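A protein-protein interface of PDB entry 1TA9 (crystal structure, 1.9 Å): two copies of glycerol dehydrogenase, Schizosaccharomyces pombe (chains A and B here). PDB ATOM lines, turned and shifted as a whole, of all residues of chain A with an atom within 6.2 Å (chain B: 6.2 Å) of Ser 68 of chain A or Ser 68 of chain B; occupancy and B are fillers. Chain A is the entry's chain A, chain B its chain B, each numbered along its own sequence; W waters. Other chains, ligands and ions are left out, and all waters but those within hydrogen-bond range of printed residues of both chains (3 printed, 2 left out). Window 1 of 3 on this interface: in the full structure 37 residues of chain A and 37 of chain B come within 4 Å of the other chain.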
ATOM      1  N   PHE A  66      15.480   5.833   0.087  1.00  0.00           N
ATOM      2  CA  PHE A  66      16.546   6.163   1.034  1.00  0.00           C
ATOM      3  C   PHE A  66      16.346   5.240   2.232  1.00  0.00           C
ATOM      4  O   PHE A  66      15.227   5.092   2.729  1.00  0.00           O
ATOM      5  CB  PHE A  66      16.454   7.622   1.494  1.00  0.00           C
ATOM      6  CG  PHE A  66      17.529   8.018   2.480  1.00  0.00           C
ATOM      7  CD1 PHE A  66      17.315   7.913   3.852  1.00  0.00           C
ATOM      8  CD2 PHE A  66      18.762   8.482   2.033  1.00  0.00           C
ATOM      9  CE1 PHE A  66      18.318   8.264   4.763  1.00  0.00           C
ATOM     10  CE2 PHE A  66      19.771   8.835   2.931  1.00  0.00           C
ATOM     11  CZ  PHE A  66      19.545   8.724   4.301  1.00  0.00           C
ATOM     12  N   THR A  67      17.426   4.619   2.693  1.00  0.00           N
ATOM     13  CA  THR A  67      17.344   3.693   3.819  1.00  0.00           C
ATOM     14  C   THR A  67      18.401   4.054   4.857  1.00  0.00           C
ATOM     15  O   THR A  67      19.434   4.633   4.519  1.00  0.00           O
ATOM     16  CB  THR A  67      17.564   2.234   3.333  1.00  0.00           C
ATOM     17  OG1 THR A  67      17.236   1.317   4.382  1.00  0.00           O
ATOM     18  CG2 THR A  67      19.016   2.020   2.913  1.00  0.00           C
ATOM     19  N   SER A  68      18.127   3.733   6.120  1.00  0.00           N
ATOM     20  CA  SER A  68      19.053   4.061   7.198  1.00  0.00           C
ATOM     21  C   SER A  68      18.660   3.471   8.550  1.00  0.00           C
ATOM     22  O   SER A  68      17.507   3.088   8.763  1.00  0.00           O
ATOM     23  CB  SER A  68      19.144   5.587   7.338  1.00  0.00           C
ATOM     24  OG  SER A  68      19.580   5.972   8.629  1.00  0.00           O
ATOM     25  N   PRO A  69      19.627   3.375   9.480  1.00  0.00           N
ATOM     26  CA  PRO A  69      19.319   2.835  10.808  1.00  0.00           C
ATOM     27  C   PRO A  69      18.411   3.907  11.416  1.00  0.00           C
ATOM     28  O   PRO A  69      18.354   5.029  10.904  1.00  0.00           O
ATOM     29  CB  PRO A  69      20.679   2.813  11.501  1.00  0.00           C
ATOM     30  CG  PRO A  69      21.658   2.693  10.364  1.00  0.00           C
ATOM     31  CD  PRO A  69      21.074   3.624   9.334  1.00  0.00           C
ATOM     32  N   GLN A  70      17.719   3.587  12.501  1.00  0.00           N
ATOM     33  CA  GLN A  70      16.846   4.569  13.127  1.00  0.00           C
ATOM     34  C   GLN A  70      17.664   5.600  13.898  1.00  0.00           C
ATOM     35  O   GLN A  70      17.304   6.776  13.958  1.00  0.00           O
ATOM     36  CB  GLN A  70      15.870   3.874  14.079  1.00  0.00           C
ATOM     37  CG  GLN A  70      14.862   2.980  13.385  1.00  0.00           C
ATOM     38  CD  GLN A  70      13.842   2.406  14.350  1.00  0.00           C
ATOM     39  OE1 GLN A  70      14.157   1.523  15.155  1.00  0.00           O
ATOM     40  NE2 GLN A  70      12.614   2.915  14.287  1.00  0.00           N
ATOM     41  N   LYS A  71      18.761   5.142  14.491  1.00  0.00           N
ATOM     42  CA  LYS A  71      19.628   6.007  15.277  1.00  0.00           C
ATOM     43  C   LYS A  71      21.098   5.639  15.105  1.00  0.00           C
ATOM     44  O   LYS A  71      21.444   4.469  14.925  1.00  0.00           O
ATOM     45  CB  LYS A  71      19.282   5.891  16.769  1.00  0.00           C
ATOM     46  CG  LYS A  71      17.847   6.225  17.146  1.00  0.00           C
ATOM     47  CD  LYS A  71      17.604   7.721  17.146  1.00  0.00           C
ATOM     48  CE  LYS A  71      16.211   8.045  17.659  1.00  0.00           C
ATOM     49  NZ  LYS A  71      15.937   9.502  17.626  1.00  0.00           N
ATOM     50  N   THR A 185      26.318   0.058   9.778  1.00  0.00           N
ATOM     51  CA  THR A 185      24.965   0.534   9.502  1.00  0.00           C
ATOM     52  C   THR A 185      24.198  -0.180   8.393  1.00  0.00           C
ATOM     53  O   THR A 185      22.986   0.016   8.265  1.00  0.00           O
ATOM     54  CB  THR A 185      24.975   2.029   9.121  1.00  0.00           C
ATOM     55  OG1 THR A 185      25.643   2.186   7.863  1.00  0.00           O
ATOM     56  CG2 THR A 185      25.695   2.860  10.180  1.00  0.00           C
ATOM     57  N   ASN A 207      17.496  -1.884   8.021  1.00  0.00           N
ATOM     58  CA  ASN A 207      18.838  -1.673   8.566  1.00  0.00           C
ATOM     59  C   ASN A 207      18.828  -1.897  10.067  1.00  0.00           C
ATOM     60  O   ASN A 207      17.773  -1.835  10.704  1.00  0.00           O
ATOM     61  CB  ASN A 207      19.316  -0.231   8.339  1.00  0.00           C
ATOM     62  CG  ASN A 207      19.557   0.093   6.883  1.00  0.00           C
ATOM     63  OD1 ASN A 207      18.630   0.119   6.080  1.00  0.00           O
ATOM     64  ND2 ASN A 207      20.811   0.344   6.539  1.00  0.00           N
ATOM     65  N   PRO A 208      20.007  -2.158  10.658  1.00  0.00           N
ATOM     66  CA  PRO A 208      20.062  -2.364  12.108  1.00  0.00           C
ATOM     67  C   PRO A 208      19.421  -1.111  12.694  1.00  0.00           C
ATOM     68  O   PRO A 208      19.555  -0.027  12.127  1.00  0.00           O
ATOM     69  CB  PRO A 208      21.557  -2.431  12.386  1.00  0.00           C
ATOM     70  CG  PRO A 208      22.092  -3.056  11.138  1.00  0.00           C
ATOM     71  CD  PRO A 208      21.336  -2.335  10.048  1.00  0.00           C
ATOM     72  N   LEU A 300      29.079   6.266   9.728  1.00  0.00           N
ATOM     73  CA  LEU A 300      27.795   6.804   9.300  1.00  0.00           C
ATOM     74  C   LEU A 300      27.763   7.256   7.845  1.00  0.00           C
ATOM     75  O   LEU A 300      26.945   6.775   7.062  1.00  0.00           O
ATOM     76  CB  LEU A 300      27.379   7.973  10.194  1.00  0.00           C
ATOM     77  CG  LEU A 300      26.059   8.650   9.811  1.00  0.00           C
ATOM     78  CD1 LEU A 300      24.915   7.651   9.923  1.00  0.00           C
ATOM     79  CD2 LEU A 300      25.814   9.847  10.712  1.00  0.00           C
ATOM     80  N   LEU A 304      25.885   5.141   4.961  1.00  0.00           N
ATOM     81  CA  LEU A 304      24.705   5.643   4.268  1.00  0.00           C
ATOM     82  C   LEU A 304      25.022   5.983   2.815  1.00  0.00           C
ATOM     83  O   LEU A 304      24.195   5.780   1.929  1.00  0.00           O
ATOM     84  CB  LEU A 304      24.152   6.887   4.970  1.00  0.00           C
ATOM     85  CG  LEU A 304      23.547   6.679   6.361  1.00  0.00           C
ATOM     86  CD1 LEU A 304      22.968   7.992   6.870  1.00  0.00           C
ATOM     87  CD2 LEU A 304      22.463   5.612   6.292  1.00  0.00           C
ATOM     88  N   GLU A 307      25.218   2.476   0.738  1.00  0.00           N
ATOM     89  CA  GLU A 307      23.953   1.748   0.648  1.00  0.00           C
ATOM     90  C   GLU A 307      22.878   2.514  -0.122  1.00  0.00           C
ATOM     91  O   GLU A 307      22.073   1.915  -0.841  1.00  0.00           O
ATOM     92  CB  GLU A 307      23.436   1.382   2.044  1.00  0.00           C
ATOM     93  CG  GLU A 307      22.297   0.371   2.011  1.00  0.00           C
ATOM     94  CD  GLU A 307      21.996  -0.240   3.374  1.00  0.00           C
ATOM     95  OE1 GLU A 307      21.111  -1.112   3.447  1.00  0.00           O
ATOM     96  OE2 GLU A 307      22.640   0.147   4.368  1.00  0.00           O
ATOM     97  N   ASN A 308      22.863   3.838   0.019  1.00  0.00           N
ATOM     98  CA  ASN A 308      21.880   4.653  -0.690  1.00  0.00           C
ATOM     99  C   ASN A 308      22.366   5.008  -2.079  1.00  0.00           C
ATOM    100  O   ASN A 308      21.617   5.530  -2.909  1.00  0.00           O
ATOM    101  CB  ASN A 308      21.557   5.904   0.117  1.00  0.00           C
ATOM    102  CG  ASN A 308      20.648   5.600   1.280  1.00  0.00           C
ATOM    103  OD1 ASN A 308      19.491   5.219   1.090  1.00  0.00           O
ATOM    104  ND2 ASN A 308      21.165   5.739   2.490  1.00  0.00           N
ATOM    105  N   PHE B  66      22.607  11.020  15.036  1.00  0.00           N
ATOM    106  CA  PHE B  66      21.918  11.158  13.757  1.00  0.00           C
ATOM    107  C   PHE B  66      20.667  10.303  13.903  1.00  0.00           C
ATOM    108  O   PHE B  66      20.728   9.187  14.429  1.00  0.00           O
ATOM    109  CB  PHE B  66      22.790  10.649  12.604  1.00  0.00           C
ATOM    110  CG  PHE B  66      22.115  10.700  11.257  1.00  0.00           C
ATOM    111  CD1 PHE B  66      21.365   9.623  10.795  1.00  0.00           C
ATOM    112  CD2 PHE B  66      22.230  11.830  10.449  1.00  0.00           C
ATOM    113  CE1 PHE B  66      20.735   9.668   9.543  1.00  0.00           C
ATOM    114  CE2 PHE B  66      21.608  11.890   9.198  1.00  0.00           C
ATOM    115  CZ  PHE B  66      20.860  10.808   8.743  1.00  0.00           C
ATOM    116  N   THR B  67      19.533  10.829  13.455  1.00  0.00           N
ATOM    117  CA  THR B  67      18.268  10.118  13.577  1.00  0.00           C
ATOM    118  C   THR B  67      17.539  10.113  12.235  1.00  0.00           C
ATOM    119  O   THR B  67      17.634  11.067  11.463  1.00  0.00           O
ATOM    120  CB  THR B  67      17.398  10.778  14.679  1.00  0.00           C
ATOM    121  OG1 THR B  67      16.251   9.965  14.946  1.00  0.00           O
ATOM    122  CG2 THR B  67      16.958  12.167  14.253  1.00  0.00           C
ATOM    123  N   SER B  68      16.815   9.037  11.948  1.00  0.00           N
ATOM    124  CA  SER B  68      16.126   8.951  10.667  1.00  0.00           C
ATOM    125  C   SER B  68      15.030   7.903  10.589  1.00  0.00           C
ATOM    126  O   SER B  68      14.923   7.025  11.449  1.00  0.00           O
ATOM    127  CB  SER B  68      17.166   8.648   9.576  1.00  0.00           C
ATOM    128  OG  SER B  68      16.565   8.238   8.361  1.00  0.00           O
ATOM    129  N   PRO B  69      14.158   8.018   9.576  1.00  0.00           N
ATOM    130  CA  PRO B  69      13.100   7.019   9.428  1.00  0.00           C
ATOM    131  C   PRO B  69      13.876   5.825   8.875  1.00  0.00           C
ATOM    132  O   PRO B  69      14.985   6.002   8.353  1.00  0.00           O
ATOM    133  CB  PRO B  69      12.191   7.623   8.362  1.00  0.00           C
ATOM    134  CG  PRO B  69      12.379   9.114   8.554  1.00  0.00           C
ATOM    135  CD  PRO B  69      13.871   9.217   8.764  1.00  0.00           C
ATOM    136  N   GLN B  70      13.324   4.624   8.978  1.00  0.00           N
ATOM    137  CA  GLN B  70      14.020   3.459   8.448  1.00  0.00           C
ATOM    138  C   GLN B  70      14.027   3.446   6.924  1.00  0.00           C
ATOM    139  O   GLN B  70      14.991   2.994   6.300  1.00  0.00           O
ATOM    140  CB  GLN B  70      13.374   2.181   8.963  1.00  0.00           C
ATOM    141  CG  GLN B  70      13.482   2.016  10.463  1.00  0.00           C
ATOM    142  CD  GLN B  70      12.842   0.737  10.941  1.00  0.00           C
ATOM    143  OE1 GLN B  70      11.613   0.609  10.960  1.00  0.00           O
ATOM    144  NE2 GLN B  70      13.671  -0.231  11.319  1.00  0.00           N
ATOM    145  N   LYS B  71      12.942   3.932   6.328  1.00  0.00           N
ATOM    146  CA  LYS B  71      12.824   3.961   4.875  1.00  0.00           C
ATOM    147  C   LYS B  71      12.053   5.185   4.397  1.00  0.00           C
ATOM    148  O   LYS B  71      11.132   5.656   5.067  1.00  0.00           O
ATOM    149  CB  LYS B  71      12.085   2.714   4.371  1.00  0.00           C
ATOM    150  CG  LYS B  71      12.737   1.378   4.696  1.00  0.00           C
ATOM    151  CD  LYS B  71      13.923   1.078   3.797  1.00  0.00           C
ATOM    152  CE  LYS B  71      14.387  -0.360   4.010  1.00  0.00           C
ATOM    153  NZ  LYS B  71      15.640  -0.682   3.274  1.00  0.00           N
ATOM    154  N   THR B 185       8.793  13.189   7.999  1.00  0.00           N
ATOM    155  CA  THR B 185       9.852  12.346   8.546  1.00  0.00           C
ATOM    156  C   THR B 185      10.235  12.560  10.002  1.00  0.00           C
ATOM    157  O   THR B 185      10.966  11.745  10.563  1.00  0.00           O
ATOM    158  CB  THR B 185      11.158  12.523   7.755  1.00  0.00           C
ATOM    159  OG1 THR B 185      11.712  13.809   8.062  1.00  0.00           O
ATOM    160  CG2 THR B 185      10.900  12.427   6.254  1.00  0.00           C
ATOM    161  N   LEU B 206      11.538   7.629  18.703  1.00  0.00           N
ATOM    162  CA  LEU B 206      12.013   7.190  17.392  1.00  0.00           C
ATOM    163  C   LEU B 206      11.251   7.907  16.281  1.00  0.00           C
ATOM    164  O   LEU B 206      10.166   8.438  16.511  1.00  0.00           O
ATOM    165  CB  LEU B 206      11.822   5.677  17.239  1.00  0.00           C
ATOM    166  CG  LEU B 206      12.534   4.763  18.243  1.00  0.00           C
ATOM    167  CD1 LEU B 206      11.942   3.362  18.165  1.00  0.00           C
ATOM    168  CD2 LEU B 206      14.024   4.740  17.954  1.00  0.00           C
ATOM    169  N   ASN B 207      11.827   7.924  15.080  1.00  0.00           N
ATOM    170  CA  ASN B 207      11.186   8.560  13.927  1.00  0.00           C
ATOM    171  C   ASN B 207      10.179   7.602  13.318  1.00  0.00           C
ATOM    172  O   ASN B 207      10.223   6.404  13.584  1.00  0.00           O
ATOM    173  CB  ASN B 207      12.214   8.884  12.836  1.00  0.00           C
ATOM    174  CG  ASN B 207      13.100  10.053  13.192  1.00  0.00           C
ATOM    175  OD1 ASN B 207      13.926   9.970  14.097  1.00  0.00           O
ATOM    176  ND2 ASN B 207      12.928  11.157  12.476  1.00  0.00           N
ATOM    177  N   PRO B 208       9.250   8.120  12.494  1.00  0.00           N
ATOM    178  CA  PRO B 208       8.268   7.231  11.867  1.00  0.00           C
ATOM    179  C   PRO B 208       9.114   6.214  11.108  1.00  0.00           C
ATOM    180  O   PRO B 208      10.217   6.538  10.664  1.00  0.00           O
ATOM    181  CB  PRO B 208       7.511   8.164  10.929  1.00  0.00           C
ATOM    182  CG  PRO B 208       7.539   9.466  11.675  1.00  0.00           C
ATOM    183  CD  PRO B 208       8.959   9.533  12.191  1.00  0.00           C
ATOM    184  N   LEU B 300      12.313  14.575   2.377  1.00  0.00           N
ATOM    185  CA  LEU B 300      13.467  13.889   2.956  1.00  0.00           C
ATOM    186  C   LEU B 300      14.602  14.811   3.392  1.00  0.00           C
ATOM    187  O   LEU B 300      15.008  14.795   4.558  1.00  0.00           O
ATOM    188  CB  LEU B 300      14.018  12.852   1.970  1.00  0.00           C
ATOM    189  CG  LEU B 300      15.238  12.038   2.417  1.00  0.00           C
ATOM    190  CD1 LEU B 300      14.882  11.159   3.611  1.00  0.00           C
ATOM    191  CD2 LEU B 300      15.722  11.185   1.256  1.00  0.00           C
ATOM    192  N   LEU B 304      15.321  15.496   7.326  1.00  0.00           N
ATOM    193  CA  LEU B 304      16.529  15.034   8.002  1.00  0.00           C
ATOM    194  C   LEU B 304      17.464  16.200   8.296  1.00  0.00           C
ATOM    195  O   LEU B 304      18.184  16.193   9.296  1.00  0.00           O
ATOM    196  CB  LEU B 304      17.270  14.011   7.141  1.00  0.00           C
ATOM    197  CG  LEU B 304      16.585  12.673   6.873  1.00  0.00           C
ATOM    198  CD1 LEU B 304      17.461  11.848   5.929  1.00  0.00           C
ATOM    199  CD2 LEU B 304      16.362  11.941   8.189  1.00  0.00           C
ATOM    200  N   GLU B 307      15.873  18.121  11.559  1.00  0.00           N
ATOM    201  CA  GLU B 307      15.879  17.340  12.791  1.00  0.00           C
ATOM    202  C   GLU B 307      17.286  16.983  13.273  1.00  0.00           C
ATOM    203  O   GLU B 307      17.542  16.930  14.482  1.00  0.00           O
ATOM    204  CB  GLU B 307      15.038  16.067  12.630  1.00  0.00           C
ATOM    205  CG  GLU B 307      14.805  15.331  13.947  1.00  0.00           C
ATOM    206  CD  GLU B 307      13.787  14.202  13.844  1.00  0.00           C
ATOM    207  OE1 GLU B 307      13.467  13.601  14.891  1.00  0.00           O
ATOM    208  OE2 GLU B 307      13.306  13.909  12.729  1.00  0.00           O
ATOM    209  N   ASN B 308      18.198  16.743  12.336  1.00  0.00           N
ATOM    210  CA  ASN B 308      19.564  16.406  12.699  1.00  0.00           C
ATOM    211  C   ASN B 308      20.399  17.648  12.913  1.00  0.00           C
ATOM    212  O   ASN B 308      21.524  17.583  13.415  1.00  0.00           O
ATOM    213  CB  ASN B 308      20.165  15.493  11.644  1.00  0.00           C
ATOM    214  CG  ASN B 308      19.616  14.091  11.748  1.00  0.00           C
ATOM    215  OD1 ASN B 308      19.863  13.397  12.738  1.00  0.00           O
ATOM    216  ND2 ASN B 308      18.844  13.674  10.752  1.00  0.00           N
HETATM  217  O   HOH W   1      16.049   0.445   6.944  1.00  0.00           O
HETATM  218  O   HOH W   2      16.495   0.876  10.650  1.00  0.00           O
HETATM  219  O   HOH W   3      13.088  10.079  17.645  1.00  0.00           O
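N of Ser 68 of chain A lies within hydrogen-bond range of O of Gln 70 of chain B.
The side-chain hydroxyl of Thr 67 of chain A is in hydrogen-bond range of the backbone carbonyl oxygen of Gln 70 of chain B, at 3.4 Å.
The backbone NH (N) of Ser 68 of chain B is in hydrogen-bond range of the backbone carbonyl oxygen (O) of Gln 70 of chain A.
The side-chain amino group (NZ) of Lys 71 of chain A lies within hydrogen-bond range of the side-chain hydroxyl (OG1) of Thr 67 of chain B.
OG1 of Thr 67 of chain A lies within hydrogen-bond range of NZ of Lys 71 of chain B (2.8 Å).
N of Thr 67 of chain B is in hydrogen-bond range of OD1 of Asn 308 of chain B.
ND2 of Asn 308 of chain B is in hydrogen-bond range of O of Leu 304 of chain B (3.0 Å).
The backbone carbonyl oxygen (O) of Leu 304 of chain A is in hydrogen-bond range of the side-chain amide nitrogen (ND2) of Asn 308 of chain A, 3.1 Å away.
The side-chain hydroxyl (OG1) of Thr 67 of chain B sits at hydrogen-bond distance from the side-chain amide oxygen (OD1) of Asn 207 of chain B (2.5 Å).
The side-chain hydroxyl of Thr 67 of chain A sits at hydrogen-bond distance from the side-chain amide oxygen of Asn 207 of chain A, at 2.5 Å.
OD1 of Asn 308 of chain A lies within hydrogen-bond range of N of Thr 67 of chain A (2.7 Å).
Among the printed residues, merely in contact across the chains: Phe 66 of chain A with Lys 71 of chain B (3.4 Å), Phe 66 of chain A with Leu 300 of chain B (3.6 Å), Phe 66 of chain A with Leu 304 of chain B (3.9 Å), Ser 68 of chain A with Phe 66 of chain B (3.98 Å), Ser 68 of chain A with Ser 68 of chain B (3.7 Å), Ser 68 of chain A with Pro 69 of chain B (3.9 Å), Gln 70 of chain A with Thr 67 of chain B (3.5 Å), Gln 70 of chain A with Gln 70 of chain B (3.4 Å), Gln 70 of chain A with Leu 206 of chain B (3.96 Å), Lys 71 of chain A with Phe 66 of chain B (3.5 Å), Lys 71 of chain A with Leu 206 of chain B (3.97 Å), Leu 300 of chain A with Phe 66 of chain B (3.7 Å) and Leu 304 of chain A with Phe 66 of chain B (3.9 Å).
Ser 68 of chain A touches just these residues of chain B: Phe 66 (3.98 Å), Ser 68 (3.7 Å), Pro 69 (3.9 Å) and Gln 70 (3.2 Å).
Of the printed residues of chain A, Ser 68 of chain B touches Ser 68 and Gln 70.
Of the printed residues of chain B, Thr 67 of chain A touches Gln 70 and Lys 71.
Printed residues of chain A within 4 Å of Gln 70 of chain B: Thr 67 (3.4 Å), Ser 68 (3.2 Å) and Gln 70 (3.4 Å).
Of the printed residues of chain A, Leu 206 of chain B touches Gln 70 and Lys 71.
Of the printed residues of chain A, Leu 300 of chain B touches Phe 66 (3.6 Å).
Of the printed residues of chain B, Leu 300 of chain A touches Phe 66 (3.7 Å).
The nearest residue of chain B that does not touch Ser 68 of chain A is Lys 71 of chain B (5.2 Å).
The nearest printed residue of chain A that does not touch Gln 70 of chain B is Phe 66 of chain A (4.1 Å).
Of the 13 printed residues of chain A, 7 touch a printed residue of chain B.
Printed residues of chain A that touch a printed residue of chain B: Phe 66, Thr 67, Ser 68, Gln 70, Lys 71, Leu 300 and Leu 304.
Hydrophobic or aromatic side chains of chain A that line the printed part of chain B: Phe 66, Leu 300 and Leu 304.
Among the printed residues, 18 pairs touch across the chains.
Among the printed residues, no Asp or Glu carboxylate lies within 4 Å of a Lys or Arg side-chain nitrogen of the other chain.
Phe 66 of chain A touches Lys 71 of chain B, and with the chains exchanged Lys 71 of chain A touches Phe 66 of chain B.
Phe 66 of chain A touches Leu 300 of chain B, and with the chains exchanged Leu 300 of chain A touches Phe 66 of chain B.
Thr 67 of chain A touches Gln 70 of chain B, and with the chains exchanged Gln 70 of chain A touches Thr 67 of chain B.
Thr 67 of chain A touches Lys 71 of chain B, and with the chains exchanged Lys 71 of chain A touches Thr 67 of chain B.
Water W1 lies within hydrogen-bond range of the side-chain amide oxygen of Asn 207 of chain A (2.7 Å), the backbone carbonyl oxygen of Gln 70 of chain B (2.8 Å) and the side-chain hydroxyl of Thr 67 of chain A (3.0 Å).
Water W3 bridges the side-chain amino group (NZ) of Lys 71 of chain A (2.9 Å) and the backbone NH (N) of Leu 206 of chain B (3.1 Å).
Water W2 lies within hydrogen-bond range of O of Asn 207 of chain A, O of Ser 68 of chain A and NE2 of Gln 70 of chain B.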
